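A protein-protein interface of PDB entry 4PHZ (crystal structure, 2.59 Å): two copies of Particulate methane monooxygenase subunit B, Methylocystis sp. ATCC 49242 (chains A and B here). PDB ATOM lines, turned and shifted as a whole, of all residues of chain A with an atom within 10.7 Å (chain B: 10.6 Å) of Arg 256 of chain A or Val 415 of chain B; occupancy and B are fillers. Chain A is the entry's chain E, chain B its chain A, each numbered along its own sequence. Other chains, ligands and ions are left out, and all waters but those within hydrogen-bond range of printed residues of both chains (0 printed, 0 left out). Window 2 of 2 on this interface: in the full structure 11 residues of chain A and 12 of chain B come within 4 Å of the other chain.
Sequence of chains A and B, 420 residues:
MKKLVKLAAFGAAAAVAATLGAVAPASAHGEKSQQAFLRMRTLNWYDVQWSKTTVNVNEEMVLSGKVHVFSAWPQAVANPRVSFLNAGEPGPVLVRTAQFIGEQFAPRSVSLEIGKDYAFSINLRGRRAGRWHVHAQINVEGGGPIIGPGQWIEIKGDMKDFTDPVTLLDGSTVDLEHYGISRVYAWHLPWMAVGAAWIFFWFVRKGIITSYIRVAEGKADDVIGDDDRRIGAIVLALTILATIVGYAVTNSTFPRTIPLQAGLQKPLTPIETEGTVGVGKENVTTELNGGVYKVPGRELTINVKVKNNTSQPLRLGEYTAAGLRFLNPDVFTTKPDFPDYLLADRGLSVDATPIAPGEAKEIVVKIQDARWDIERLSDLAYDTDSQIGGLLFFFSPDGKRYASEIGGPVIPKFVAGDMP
The guanidinium group (NH2) of Arg 256 of chain A is in hydrogen-bond range of the backbone carbonyl oxygen (O) of Val 415 of chain B.
OH of Tyr 293 of chain B sits close to N of Ala 381 of chain B (3.4 Å).
The backbone carbonyl oxygen (O) of Ile 411 of chain B lies within hydrogen-bond range of the backbone NH (N) of Tyr 293 of chain B (3.0 Å).
O of Val 295 of chain B is in hydrogen-bond range of N of Val 415 of chain B, at 2.9 Å.
Leu 169 of chain A touches Ile 411 of chain B (CD2 to CG2, 3.8 Å).
Leu 169 of chain A touches Pro 412 of chain B.
CB of Arg 256 of chain A touches CD2 of Phe 414 of chain B (3.6 Å).
CG2 of Ile 258 of chain A touches O of Ala 381 of chain B (3.8 Å).
CD of Pro 259 of chain A touches O of Ala 381 of chain B, 3.8 Å away.
O of Tyr 382 of chain B touches CG of Pro 259 of chain A, at 3.3 Å.
Of the printed residues of chain B, Arg 256 of chain A touches Phe 414 (3.6 Å) and Val 415 (3.0 Å).
Val 415 of chain B touches just one residue of chain A: Arg 256 (3.0 Å).
No residue of chain B comes within 4 Å of Pro 255 of chain A.
No residue of chain A comes within 4 Å of Lys 294 of chain B.
No residue of chain A comes within 4 Å of Val 295 of chain B.
Phe 414 of chain B touches just one residue of chain A: Arg 256 (3.6 Å).
Of the printed residues of chain B, Leu 169 of chain A touches Ile 411 (3.8 Å) and Pro 412 (3.3 Å).
Printed residues of chain A within 4 Å of Ala 381 of chain B: Ile 258 and Pro 259.
Printed residues of chain B within 4 Å of Pro 259 of chain A: Ala 381 and Tyr 382.
The nearest residue of chain A that does not touch Val 415 of chain B is Pro 255 of chain A (8.5 Å).
Printed residues of chain B that touch a printed residue of chain A: Ala 381, Tyr 382, Ile 411, Pro 412, Phe 414 and Val 415.
Of the 17 printed residues of chain A, 4 touch a printed residue of chain B.
Printed residues of chain A that touch a printed residue of chain B: Leu 169, Arg 256, Ile 258 and Pro 259.
Hydrophobic or aromatic side chains of chain A within 4 Å of the printed part of chain B: Leu 169, Ile 258 and Pro 259.
No position is printed for both chains.
Of the 7 pairs that touch across the chains among the printed residues, none has its exchanged pair printed and touching as well.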
ATOM      1  N   LEU A 168      30.364   7.551  23.684  1.00  0.00           N
ATOM      2  CA  LEU A 168      29.174   8.223  24.215  1.00  0.00           C
ATOM      3  C   LEU A 168      29.310   8.508  25.716  1.00  0.00           C
ATOM      4  O   LEU A 168      30.240   8.024  26.354  1.00  0.00           O
ATOM      5  CB  LEU A 168      27.937   7.376  23.915  1.00  0.00           C
ATOM      6  CG  LEU A 168      27.340   7.397  22.490  1.00  0.00           C
ATOM      7  CD1 LEU A 168      28.312   7.285  21.331  1.00  0.00           C
ATOM      8  CD2 LEU A 168      26.332   6.284  22.332  1.00  0.00           C
ATOM      9  N   LEU A 169      28.407   9.320  26.267  1.00  0.00           N
ATOM     10  CA  LEU A 169      28.419   9.665  27.683  1.00  0.00           C
ATOM     11  C   LEU A 169      28.094   8.475  28.569  1.00  0.00           C
ATOM     12  O   LEU A 169      28.604   8.361  29.688  1.00  0.00           O
ATOM     13  CB  LEU A 169      27.412  10.742  27.986  1.00  0.00           C
ATOM     14  CG  LEU A 169      27.774  12.222  28.000  1.00  0.00           C
ATOM     15  CD1 LEU A 169      26.800  12.931  28.934  1.00  0.00           C
ATOM     16  CD2 LEU A 169      29.192  12.556  28.432  1.00  0.00           C
ATOM     17  N   ASP A 170      27.233   7.592  28.068  1.00  0.00           N
ATOM     18  CA  ASP A 170      26.862   6.369  28.781  1.00  0.00           C
ATOM     19  C   ASP A 170      28.017   5.347  28.842  1.00  0.00           C
ATOM     20  O   ASP A 170      27.875   4.297  29.473  1.00  0.00           O
ATOM     21  CB  ASP A 170      25.632   5.750  28.117  1.00  0.00           C
ATOM     22  CG  ASP A 170      25.939   5.137  26.749  1.00  0.00           C
ATOM     23  OD1 ASP A 170      27.134   4.958  26.380  1.00  0.00           O
ATOM     24  OD2 ASP A 170      24.962   4.813  26.041  1.00  0.00           O
ATOM     25  N   SER A 172      29.511   3.636  26.198  1.00  0.00           N
ATOM     26  CA  SER A 172      29.639   2.804  24.986  1.00  0.00           C
ATOM     27  C   SER A 172      30.344   3.473  23.791  1.00  0.00           C
ATOM     28  O   SER A 172      30.361   4.694  23.653  1.00  0.00           O
ATOM     29  CB  SER A 172      28.271   2.295  24.545  1.00  0.00           C
ATOM     30  OG  SER A 172      27.374   3.366  24.417  1.00  0.00           O
ATOM     31  N   TYR A 179      27.796   4.526  12.141  1.00  0.00           N
ATOM     32  CA  TYR A 179      26.785   4.609  13.185  1.00  0.00           C
ATOM     33  C   TYR A 179      25.549   5.392  12.736  1.00  0.00           C
ATOM     34  O   TYR A 179      25.674   6.512  12.232  1.00  0.00           O
ATOM     35  CB  TYR A 179      27.306   5.218  14.472  1.00  0.00           C
ATOM     36  CG  TYR A 179      26.241   5.189  15.554  1.00  0.00           C
ATOM     37  CD1 TYR A 179      25.747   3.975  16.035  1.00  0.00           C
ATOM     38  CD2 TYR A 179      25.699   6.381  16.089  1.00  0.00           C
ATOM     39  CE1 TYR A 179      24.767   3.937  17.021  1.00  0.00           C
ATOM     40  CE2 TYR A 179      24.706   6.345  17.081  1.00  0.00           C
ATOM     41  CZ  TYR A 179      24.255   5.117  17.542  1.00  0.00           C
ATOM     42  OH  TYR A 179      23.281   5.063  18.517  1.00  0.00           O
ATOM     43  N   ALA A 248       7.531   6.562  19.847  1.00  0.00           N
ATOM     44  CA  ALA A 248       7.684   5.909  21.162  1.00  0.00           C
ATOM     45  C   ALA A 248       8.832   4.877  21.235  1.00  0.00           C
ATOM     46  O   ALA A 248       9.600   4.881  22.187  1.00  0.00           O
ATOM     47  CB  ALA A 248       6.379   5.282  21.582  1.00  0.00           C
ATOM     48  N   VAL A 249       8.956   4.006  20.237  1.00  0.00           N
ATOM     49  CA  VAL A 249      10.092   3.076  20.183  1.00  0.00           C
ATOM     50  C   VAL A 249      11.404   3.853  20.208  1.00  0.00           C
ATOM     51  O   VAL A 249      12.188   3.698  21.153  1.00  0.00           O
ATOM     52  CB  VAL A 249      10.038   2.154  18.945  1.00  0.00           C
ATOM     53  CG1 VAL A 249      11.385   1.537  18.638  1.00  0.00           C
ATOM     54  CG2 VAL A 249       8.987   1.085  19.136  1.00  0.00           C
ATOM     55  N   THR A 250      11.654   4.687  19.194  1.00  0.00           N
ATOM     56  CA  THR A 250      12.921   5.439  19.149  1.00  0.00           C
ATOM     57  C   THR A 250      13.145   6.249  20.432  1.00  0.00           C
ATOM     58  O   THR A 250      14.274   6.612  20.738  1.00  0.00           O
ATOM     59  CB  THR A 250      13.099   6.353  17.902  1.00  0.00           C
ATOM     60  OG1 THR A 250      11.982   7.237  17.779  1.00  0.00           O
ATOM     61  CG2 THR A 250      13.300   5.522  16.634  1.00  0.00           C
ATOM     62  N   ASN A 251      12.073   6.509  21.171  1.00  0.00           N
ATOM     63  CA  ASN A 251      12.160   7.189  22.438  1.00  0.00           C
ATOM     64  C   ASN A 251      12.662   6.292  23.563  1.00  0.00           C
ATOM     65  O   ASN A 251      13.207   6.775  24.559  1.00  0.00           O
ATOM     66  CB  ASN A 251      10.798   7.690  22.795  1.00  0.00           C
ATOM     67  CG  ASN A 251      10.831   9.079  23.340  1.00  0.00           C
ATOM     68  OD1 ASN A 251      11.630   9.907  22.903  1.00  0.00           O
ATOM     69  ND2 ASN A 251       9.943   9.359  24.285  1.00  0.00           N
ATOM     70  N   SER A 252      12.469   4.981  23.392  1.00  0.00           N
ATOM     71  CA  SER A 252      12.899   3.958  24.363  1.00  0.00           C
ATOM     72  C   SER A 252      14.346   3.583  24.122  1.00  0.00           C
ATOM     73  O   SER A 252      15.160   3.737  25.042  1.00  0.00           O
ATOM     74  CB  SER A 252      12.007   2.713  24.312  1.00  0.00           C
ATOM     75  OG  SER A 252      10.815   2.947  25.038  1.00  0.00           O
ATOM     76  N   THR A 253      14.691   3.111  22.915  1.00  0.00           N
ATOM     77  CA  THR A 253      16.091   3.207  22.499  1.00  0.00           C
ATOM     78  C   THR A 253      16.323   4.672  22.801  1.00  0.00           C
ATOM     79  O   THR A 253      15.362   5.414  22.882  1.00  0.00           O
ATOM     80  CB  THR A 253      16.249   3.001  20.980  1.00  0.00           C
ATOM     81  OG1 THR A 253      15.268   2.074  20.494  1.00  0.00           O
ATOM     82  CG2 THR A 253      17.648   2.523  20.624  1.00  0.00           C
ATOM     83  N   PHE A 254      17.537   5.135  22.993  1.00  0.00           N
ATOM     84  CA  PHE A 254      17.736   6.617  23.087  1.00  0.00           C
ATOM     85  C   PHE A 254      16.791   7.425  23.972  1.00  0.00           C
ATOM     86  O   PHE A 254      16.190   8.357  23.465  1.00  0.00           O
ATOM     87  CB  PHE A 254      17.685   7.293  21.696  1.00  0.00           C
ATOM     88  CG  PHE A 254      18.299   6.487  20.616  1.00  0.00           C
ATOM     89  CD1 PHE A 254      19.611   6.042  20.712  1.00  0.00           C
ATOM     90  CD2 PHE A 254      17.569   6.186  19.492  1.00  0.00           C
ATOM     91  CE1 PHE A 254      20.175   5.282  19.699  1.00  0.00           C
ATOM     92  CE2 PHE A 254      18.131   5.440  18.460  1.00  0.00           C
ATOM     93  CZ  PHE A 254      19.434   4.984  18.558  1.00  0.00           C
ATOM     94  N   PRO A 255      16.701   7.128  25.283  1.00  0.00           N
ATOM     95  CA  PRO A 255      15.836   7.975  26.127  1.00  0.00           C
ATOM     96  C   PRO A 255      16.462   9.281  26.661  1.00  0.00           C
ATOM     97  O   PRO A 255      15.776  10.033  27.332  1.00  0.00           O
ATOM     98  CB  PRO A 255      15.545   7.074  27.308  1.00  0.00           C
ATOM     99  CG  PRO A 255      16.808   6.299  27.462  1.00  0.00           C
ATOM    100  CD  PRO A 255      17.402   6.114  26.088  1.00  0.00           C
ATOM    101  N   ARG A 256      17.747   9.523  26.411  1.00  0.00           N
ATOM    102  CA  ARG A 256      18.386  10.777  26.832  1.00  0.00           C
ATOM    103  C   ARG A 256      19.170  11.433  25.692  1.00  0.00           C
ATOM    104  O   ARG A 256      20.233  10.947  25.294  1.00  0.00           O
ATOM    105  CB  ARG A 256      19.315  10.551  28.036  1.00  0.00           C
ATOM    106  CG  ARG A 256      18.635  10.409  29.397  1.00  0.00           C
ATOM    107  CD  ARG A 256      18.435   8.938  29.737  1.00  0.00           C
ATOM    108  NE  ARG A 256      18.646   8.613  31.152  1.00  0.00           N
ATOM    109  CZ  ARG A 256      18.727   7.367  31.629  1.00  0.00           C
ATOM    110  NH1 ARG A 256      18.616   6.324  30.809  1.00  0.00           N
ATOM    111  NH2 ARG A 256      18.927   7.159  32.928  1.00  0.00           N
ATOM    112  N   THR A 257      18.636  12.528  25.168  1.00  0.00           N
ATOM    113  CA  THR A 257      19.223  13.208  24.022  1.00  0.00           C
ATOM    114  C   THR A 257      19.345  14.709  24.311  1.00  0.00           C
ATOM    115  O   THR A 257      18.648  15.269  25.175  1.00  0.00           O
ATOM    116  CB  THR A 257      18.434  12.975  22.694  1.00  0.00           C
ATOM    117  OG1 THR A 257      17.021  13.079  22.901  1.00  0.00           O
ATOM    118  CG2 THR A 257      18.722  11.608  22.092  1.00  0.00           C
ATOM    119  N   ILE A 258      20.242  15.361  23.587  1.00  0.00           N
ATOM    120  CA  ILE A 258      20.496  16.776  23.798  1.00  0.00           C
ATOM    121  C   ILE A 258      20.273  17.517  22.467  1.00  0.00           C
ATOM    122  O   ILE A 258      20.350  16.882  21.383  1.00  0.00           O
ATOM    123  CB  ILE A 258      21.932  17.012  24.349  1.00  0.00           C
ATOM    124  CG1 ILE A 258      22.960  16.103  23.644  1.00  0.00           C
ATOM    125  CG2 ILE A 258      21.969  16.767  25.846  1.00  0.00           C
ATOM    126  CD1 ILE A 258      24.371  16.657  23.628  1.00  0.00           C
ATOM    127  N   PRO A 259      19.972  18.842  22.535  1.00  0.00           N
ATOM    128  CA  PRO A 259      19.895  19.647  21.313  1.00  0.00           C
ATOM    129  C   PRO A 259      21.286  19.905  20.726  1.00  0.00           C
ATOM    130  O   PRO A 259      22.252  19.935  21.485  1.00  0.00           O
ATOM    131  CB  PRO A 259      19.275  20.965  21.804  1.00  0.00           C
ATOM    132  CG  PRO A 259      19.574  21.023  23.262  1.00  0.00           C
ATOM    133  CD  PRO A 259      19.590  19.613  23.739  1.00  0.00           C
ATOM    134  N   VAL B 292      30.358  18.374  36.501  1.00  0.00           N
ATOM    135  CA  VAL B 292      29.326  17.380  36.270  1.00  0.00           C
ATOM    136  C   VAL B 292      28.045  17.780  37.013  1.00  0.00           C
ATOM    137  O   VAL B 292      28.111  18.256  38.144  1.00  0.00           O
ATOM    138  CB  VAL B 292      29.815  15.946  36.566  1.00  0.00           C
ATOM    139  CG1 VAL B 292      28.669  14.965  36.491  1.00  0.00           C
ATOM    140  CG2 VAL B 292      30.854  15.523  35.550  1.00  0.00           C
ATOM    141  N   TYR B 293      26.902  17.657  36.336  1.00  0.00           N
ATOM    142  CA  TYR B 293      25.601  17.884  36.946  1.00  0.00           C
ATOM    143  C   TYR B 293      24.710  16.682  36.685  1.00  0.00           C
ATOM    144  O   TYR B 293      24.833  16.005  35.655  1.00  0.00           O
ATOM    145  CB  TYR B 293      24.957  19.219  36.503  1.00  0.00           C
ATOM    146  CG  TYR B 293      24.578  19.340  35.032  1.00  0.00           C
ATOM    147  CD1 TYR B 293      25.560  19.452  34.033  1.00  0.00           C
ATOM    148  CD2 TYR B 293      23.231  19.382  34.633  1.00  0.00           C
ATOM    149  CE1 TYR B 293      25.208  19.571  32.689  1.00  0.00           C
ATOM    150  CE2 TYR B 293      22.875  19.495  33.288  1.00  0.00           C
ATOM    151  CZ  TYR B 293      23.861  19.588  32.326  1.00  0.00           C
ATOM    152  OH  TYR B 293      23.504  19.697  31.008  1.00  0.00           O
ATOM    153  N   LYS B 294      23.835  16.405  37.645  1.00  0.00           N
ATOM    154  CA  LYS B 294      22.963  15.250  37.553  1.00  0.00           C
ATOM    155  C   LYS B 294      21.604  15.611  36.980  1.00  0.00           C
ATOM    156  O   LYS B 294      20.976  16.620  37.352  1.00  0.00           O
ATOM    157  CB  LYS B 294      22.828  14.568  38.910  1.00  0.00           C
ATOM    158  CG  LYS B 294      23.980  13.629  39.199  1.00  0.00           C
ATOM    159  CD  LYS B 294      23.991  13.185  40.643  1.00  0.00           C
ATOM    160  CE  LYS B 294      25.268  12.430  40.939  1.00  0.00           C
ATOM    161  NZ  LYS B 294      25.055  11.534  42.105  1.00  0.00           N
ATOM    162  N   VAL B 295      21.183  14.763  36.053  1.00  0.00           N
ATOM    163  CA  VAL B 295      19.951  14.909  35.311  1.00  0.00           C
ATOM    164  C   VAL B 295      19.216  13.577  35.461  1.00  0.00           C
ATOM    165  O   VAL B 295      19.721  12.542  34.997  1.00  0.00           O
ATOM    166  CB  VAL B 295      20.243  15.177  33.813  1.00  0.00           C
ATOM    167  CG1 VAL B 295      18.950  15.262  33.010  1.00  0.00           C
ATOM    168  CG2 VAL B 295      21.100  16.428  33.642  1.00  0.00           C
ATOM    169  N   PRO B 296      18.063  13.583  36.161  1.00  0.00           N
ATOM    170  CA  PRO B 296      17.572  14.736  36.939  1.00  0.00           C
ATOM    171  C   PRO B 296      18.394  14.900  38.206  1.00  0.00           C
ATOM    172  O   PRO B 296      19.137  13.982  38.569  1.00  0.00           O
ATOM    173  CB  PRO B 296      16.142  14.341  37.307  1.00  0.00           C
ATOM    174  CG  PRO B 296      16.116  12.849  37.214  1.00  0.00           C
ATOM    175  CD  PRO B 296      17.109  12.458  36.159  1.00  0.00           C
ATOM    176  N   GLY B 297      18.279  16.039  38.878  1.00  0.00           N
ATOM    177  CA  GLY B 297      19.038  16.205  40.087  1.00  0.00           C
ATOM    178  C   GLY B 297      19.022  17.547  40.774  1.00  0.00           C
ATOM    179  O   GLY B 297      18.220  18.427  40.461  1.00  0.00           O
ATOM    180  N   ARG B 298      19.968  17.677  41.702  1.00  0.00           N
ATOM    181  CA  ARG B 298      20.053  18.722  42.712  1.00  0.00           C
ATOM    182  C   ARG B 298      21.524  19.127  42.820  1.00  0.00           C
ATOM    183  O   ARG B 298      21.869  20.053  43.544  1.00  0.00           O
ATOM    184  CB  ARG B 298      19.635  18.080  44.034  1.00  0.00           C
ATOM    185  CG  ARG B 298      18.888  18.956  45.022  1.00  0.00           C
ATOM    186  CD  ARG B 298      17.874  18.151  45.838  1.00  0.00           C
ATOM    187  NE  ARG B 298      17.090  17.268  44.965  1.00  0.00           N
ATOM    188  CZ  ARG B 298      16.047  17.644  44.217  1.00  0.00           C
ATOM    189  NH1 ARG B 298      15.609  18.903  44.226  1.00  0.00           N
ATOM    190  NH2 ARG B 298      15.437  16.747  43.452  1.00  0.00           N
ATOM    191  N   GLU B 299      22.379  18.419  42.075  1.00  0.00           N
ATOM    192  CA  GLU B 299      23.839  18.395  42.262  1.00  0.00           C
ATOM    193  C   GLU B 299      24.678  18.966  41.119  1.00  0.00           C
ATOM    194  O   GLU B 299      24.408  18.689  39.944  1.00  0.00           O
ATOM    195  CB  GLU B 299      24.292  16.941  42.468  1.00  0.00           C
ATOM    196  CG  GLU B 299      24.557  16.565  43.913  1.00  0.00           C
ATOM    197  CD  GLU B 299      24.141  15.144  44.225  1.00  0.00           C
ATOM    198  OE1 GLU B 299      22.939  14.917  44.514  1.00  0.00           O
ATOM    199  OE2 GLU B 299      25.021  14.260  44.190  1.00  0.00           O
ATOM    200  N   LEU B 300      25.719  19.721  41.477  1.00  0.00           N
ATOM    201  CA  LEU B 300      26.760  20.112  40.525  1.00  0.00           C
ATOM    202  C   LEU B 300      28.160  20.059  41.142  1.00  0.00           C
ATOM    203  O   LEU B 300      28.439  20.709  42.140  1.00  0.00           O
ATOM    204  CB  LEU B 300      26.496  21.507  39.957  1.00  0.00           C
ATOM    205  CG  LEU B 300      27.668  22.111  39.190  1.00  0.00           C
ATOM    206  CD1 LEU B 300      27.824  21.475  37.806  1.00  0.00           C
ATOM    207  CD2 LEU B 300      27.532  23.625  39.154  1.00  0.00           C
ATOM    208  N   ASP B 373      17.375  22.678  41.448  1.00  0.00           N
ATOM    209  CA  ASP B 373      16.293  22.089  40.684  1.00  0.00           C
ATOM    210  C   ASP B 373      15.057  22.993  40.596  1.00  0.00           C
ATOM    211  O   ASP B 373      14.440  23.096  39.543  1.00  0.00           O
ATOM    212  CB  ASP B 373      15.921  20.728  41.237  1.00  0.00           C
ATOM    213  CG  ASP B 373      15.136  19.914  40.249  1.00  0.00           C
ATOM    214  OD1 ASP B 373      15.755  19.319  39.334  1.00  0.00           O
ATOM    215  OD2 ASP B 373      13.895  19.881  40.377  1.00  0.00           O
ATOM    216  N   SER B 378      18.615  23.011  36.623  1.00  0.00           N
ATOM    217  CA  SER B 378      18.857  21.628  36.155  1.00  0.00           C
ATOM    218  C   SER B 378      18.459  21.418  34.659  1.00  0.00           C
ATOM    219  O   SER B 378      18.898  20.441  33.996  1.00  0.00           O
ATOM    220  CB  SER B 378      18.142  20.618  37.075  1.00  0.00           C
ATOM    221  OG  SER B 378      16.815  21.036  37.378  1.00  0.00           O
ATOM    222  N   ALA B 381      20.263  20.811  30.736  1.00  0.00           N
ATOM    223  CA  ALA B 381      20.291  19.683  29.818  1.00  0.00           C
ATOM    224  C   ALA B 381      19.486  19.981  28.559  1.00  0.00           C
ATOM    225  O   ALA B 381      19.837  19.487  27.480  1.00  0.00           O
ATOM    226  CB  ALA B 381      19.740  18.453  30.496  1.00  0.00           C
ATOM    227  N   TYR B 382      18.411  20.767  28.718  1.00  0.00           N
ATOM    228  CA  TYR B 382      17.552  21.214  27.626  1.00  0.00           C
ATOM    229  C   TYR B 382      18.191  22.328  26.759  1.00  0.00           C
ATOM    230  O   TYR B 382      17.842  22.505  25.584  1.00  0.00           O
ATOM    231  CB  TYR B 382      16.202  21.676  28.178  1.00  0.00           C
ATOM    232  CG  TYR B 382      15.230  22.109  27.101  1.00  0.00           C
ATOM    233  CD1 TYR B 382      14.426  21.162  26.448  1.00  0.00           C
ATOM    234  CD2 TYR B 382      15.124  23.470  26.705  1.00  0.00           C
ATOM    235  CE1 TYR B 382      13.542  21.537  25.450  1.00  0.00           C
ATOM    236  CE2 TYR B 382      14.240  23.852  25.700  1.00  0.00           C
ATOM    237  CZ  TYR B 382      13.455  22.872  25.079  1.00  0.00           C
ATOM    238  OH  TYR B 382      12.560  23.201  24.091  1.00  0.00           O
ATOM    239  N   ILE B 411      29.259  18.867  32.078  1.00  0.00           N
ATOM    240  CA  ILE B 411      28.719  17.660  31.439  1.00  0.00           C
ATOM    241  C   ILE B 411      27.617  17.088  32.323  1.00  0.00           C
ATOM    242  O   ILE B 411      27.754  17.097  33.535  1.00  0.00           O
ATOM    243  CB  ILE B 411      29.806  16.597  31.206  1.00  0.00           C
ATOM    244  CG1 ILE B 411      30.511  16.823  29.885  1.00  0.00           C
ATOM    245  CG2 ILE B 411      29.216  15.211  31.189  1.00  0.00           C
ATOM    246  CD1 ILE B 411      31.444  18.000  29.882  1.00  0.00           C
ATOM    247  N   PRO B 412      26.504  16.624  31.725  1.00  0.00           N
ATOM    248  CA  PRO B 412      25.472  16.044  32.565  1.00  0.00           C
ATOM    249  C   PRO B 412      25.719  14.545  32.867  1.00  0.00           C
ATOM    250  O   PRO B 412      26.304  13.799  32.053  1.00  0.00           O
ATOM    251  CB  PRO B 412      24.224  16.230  31.712  1.00  0.00           C
ATOM    252  CG  PRO B 412      24.724  16.070  30.293  1.00  0.00           C
ATOM    253  CD  PRO B 412      26.113  16.638  30.295  1.00  0.00           C
ATOM    254  N   LYS B 413      25.264  14.104  34.033  1.00  0.00           N
ATOM    255  CA  LYS B 413      25.318  12.697  34.372  1.00  0.00           C
ATOM    256  C   LYS B 413      23.879  12.259  34.295  1.00  0.00           C
ATOM    257  O   LYS B 413      23.035  12.824  35.002  1.00  0.00           O
ATOM    258  CB  LYS B 413      25.886  12.528  35.784  1.00  0.00           C
ATOM    259  CG  LYS B 413      26.003  11.101  36.311  1.00  0.00           C
ATOM    260  CD  LYS B 413      27.247  10.399  35.803  1.00  0.00           C
ATOM    261  CE  LYS B 413      27.230   8.916  36.149  1.00  0.00           C
ATOM    262  NZ  LYS B 413      27.961   8.103  35.130  1.00  0.00           N
ATOM    263  N   PHE B 414      23.590  11.295  33.414  1.00  0.00           N
ATOM    264  CA  PHE B 414      22.207  10.845  33.214  1.00  0.00           C
ATOM    265  C   PHE B 414      21.888   9.714  34.174  1.00  0.00           C
ATOM    266  O   PHE B 414      22.242   8.546  33.953  1.00  0.00           O
ATOM    267  CB  PHE B 414      21.905  10.441  31.756  1.00  0.00           C
ATOM    268  CG  PHE B 414      21.752  11.604  30.809  1.00  0.00           C
ATOM    269  CD1 PHE B 414      20.937  12.692  31.134  1.00  0.00           C
ATOM    270  CD2 PHE B 414      22.415  11.606  29.575  1.00  0.00           C
ATOM    271  CE1 PHE B 414      20.797  13.756  30.256  1.00  0.00           C
ATOM    272  CE2 PHE B 414      22.275  12.671  28.695  1.00  0.00           C
ATOM    273  CZ  PHE B 414      21.466  13.744  29.040  1.00  0.00           C
ATOM    274  N   VAL B 415      21.212  10.087  35.249  1.00  0.00           N
ATOM    275  CA  VAL B 415      20.885   9.166  36.317  1.00  0.00           C
ATOM    276  C   VAL B 415      19.480   8.544  36.113  1.00  0.00           C
ATOM    277  O   VAL B 415      18.720   8.989  35.241  1.00  0.00           O
ATOM    278  CB  VAL B 415      21.063   9.868  37.699  1.00  0.00           C
ATOM    279  CG1 VAL B 415      22.432  10.533  37.780  1.00  0.00           C
ATOM    280  CG2 VAL B 415      19.974  10.906  37.969  1.00  0.00           C
ATOM    281  N   ALA B 416      19.154   7.520  36.912  1.00  0.00           N
ATOM    282  CA  ALA B 416      17.841   6.847  36.883  1.00  0.00           C
ATOM    283  C   ALA B 416      16.637   7.796  37.110  1.00  0.00           C
ATOM    284  O   ALA B 416      16.705   8.761  37.882  1.00  0.00           O
ATOM    285  CB  ALA B 416      17.815   5.683  37.871  1.00  0.00           C
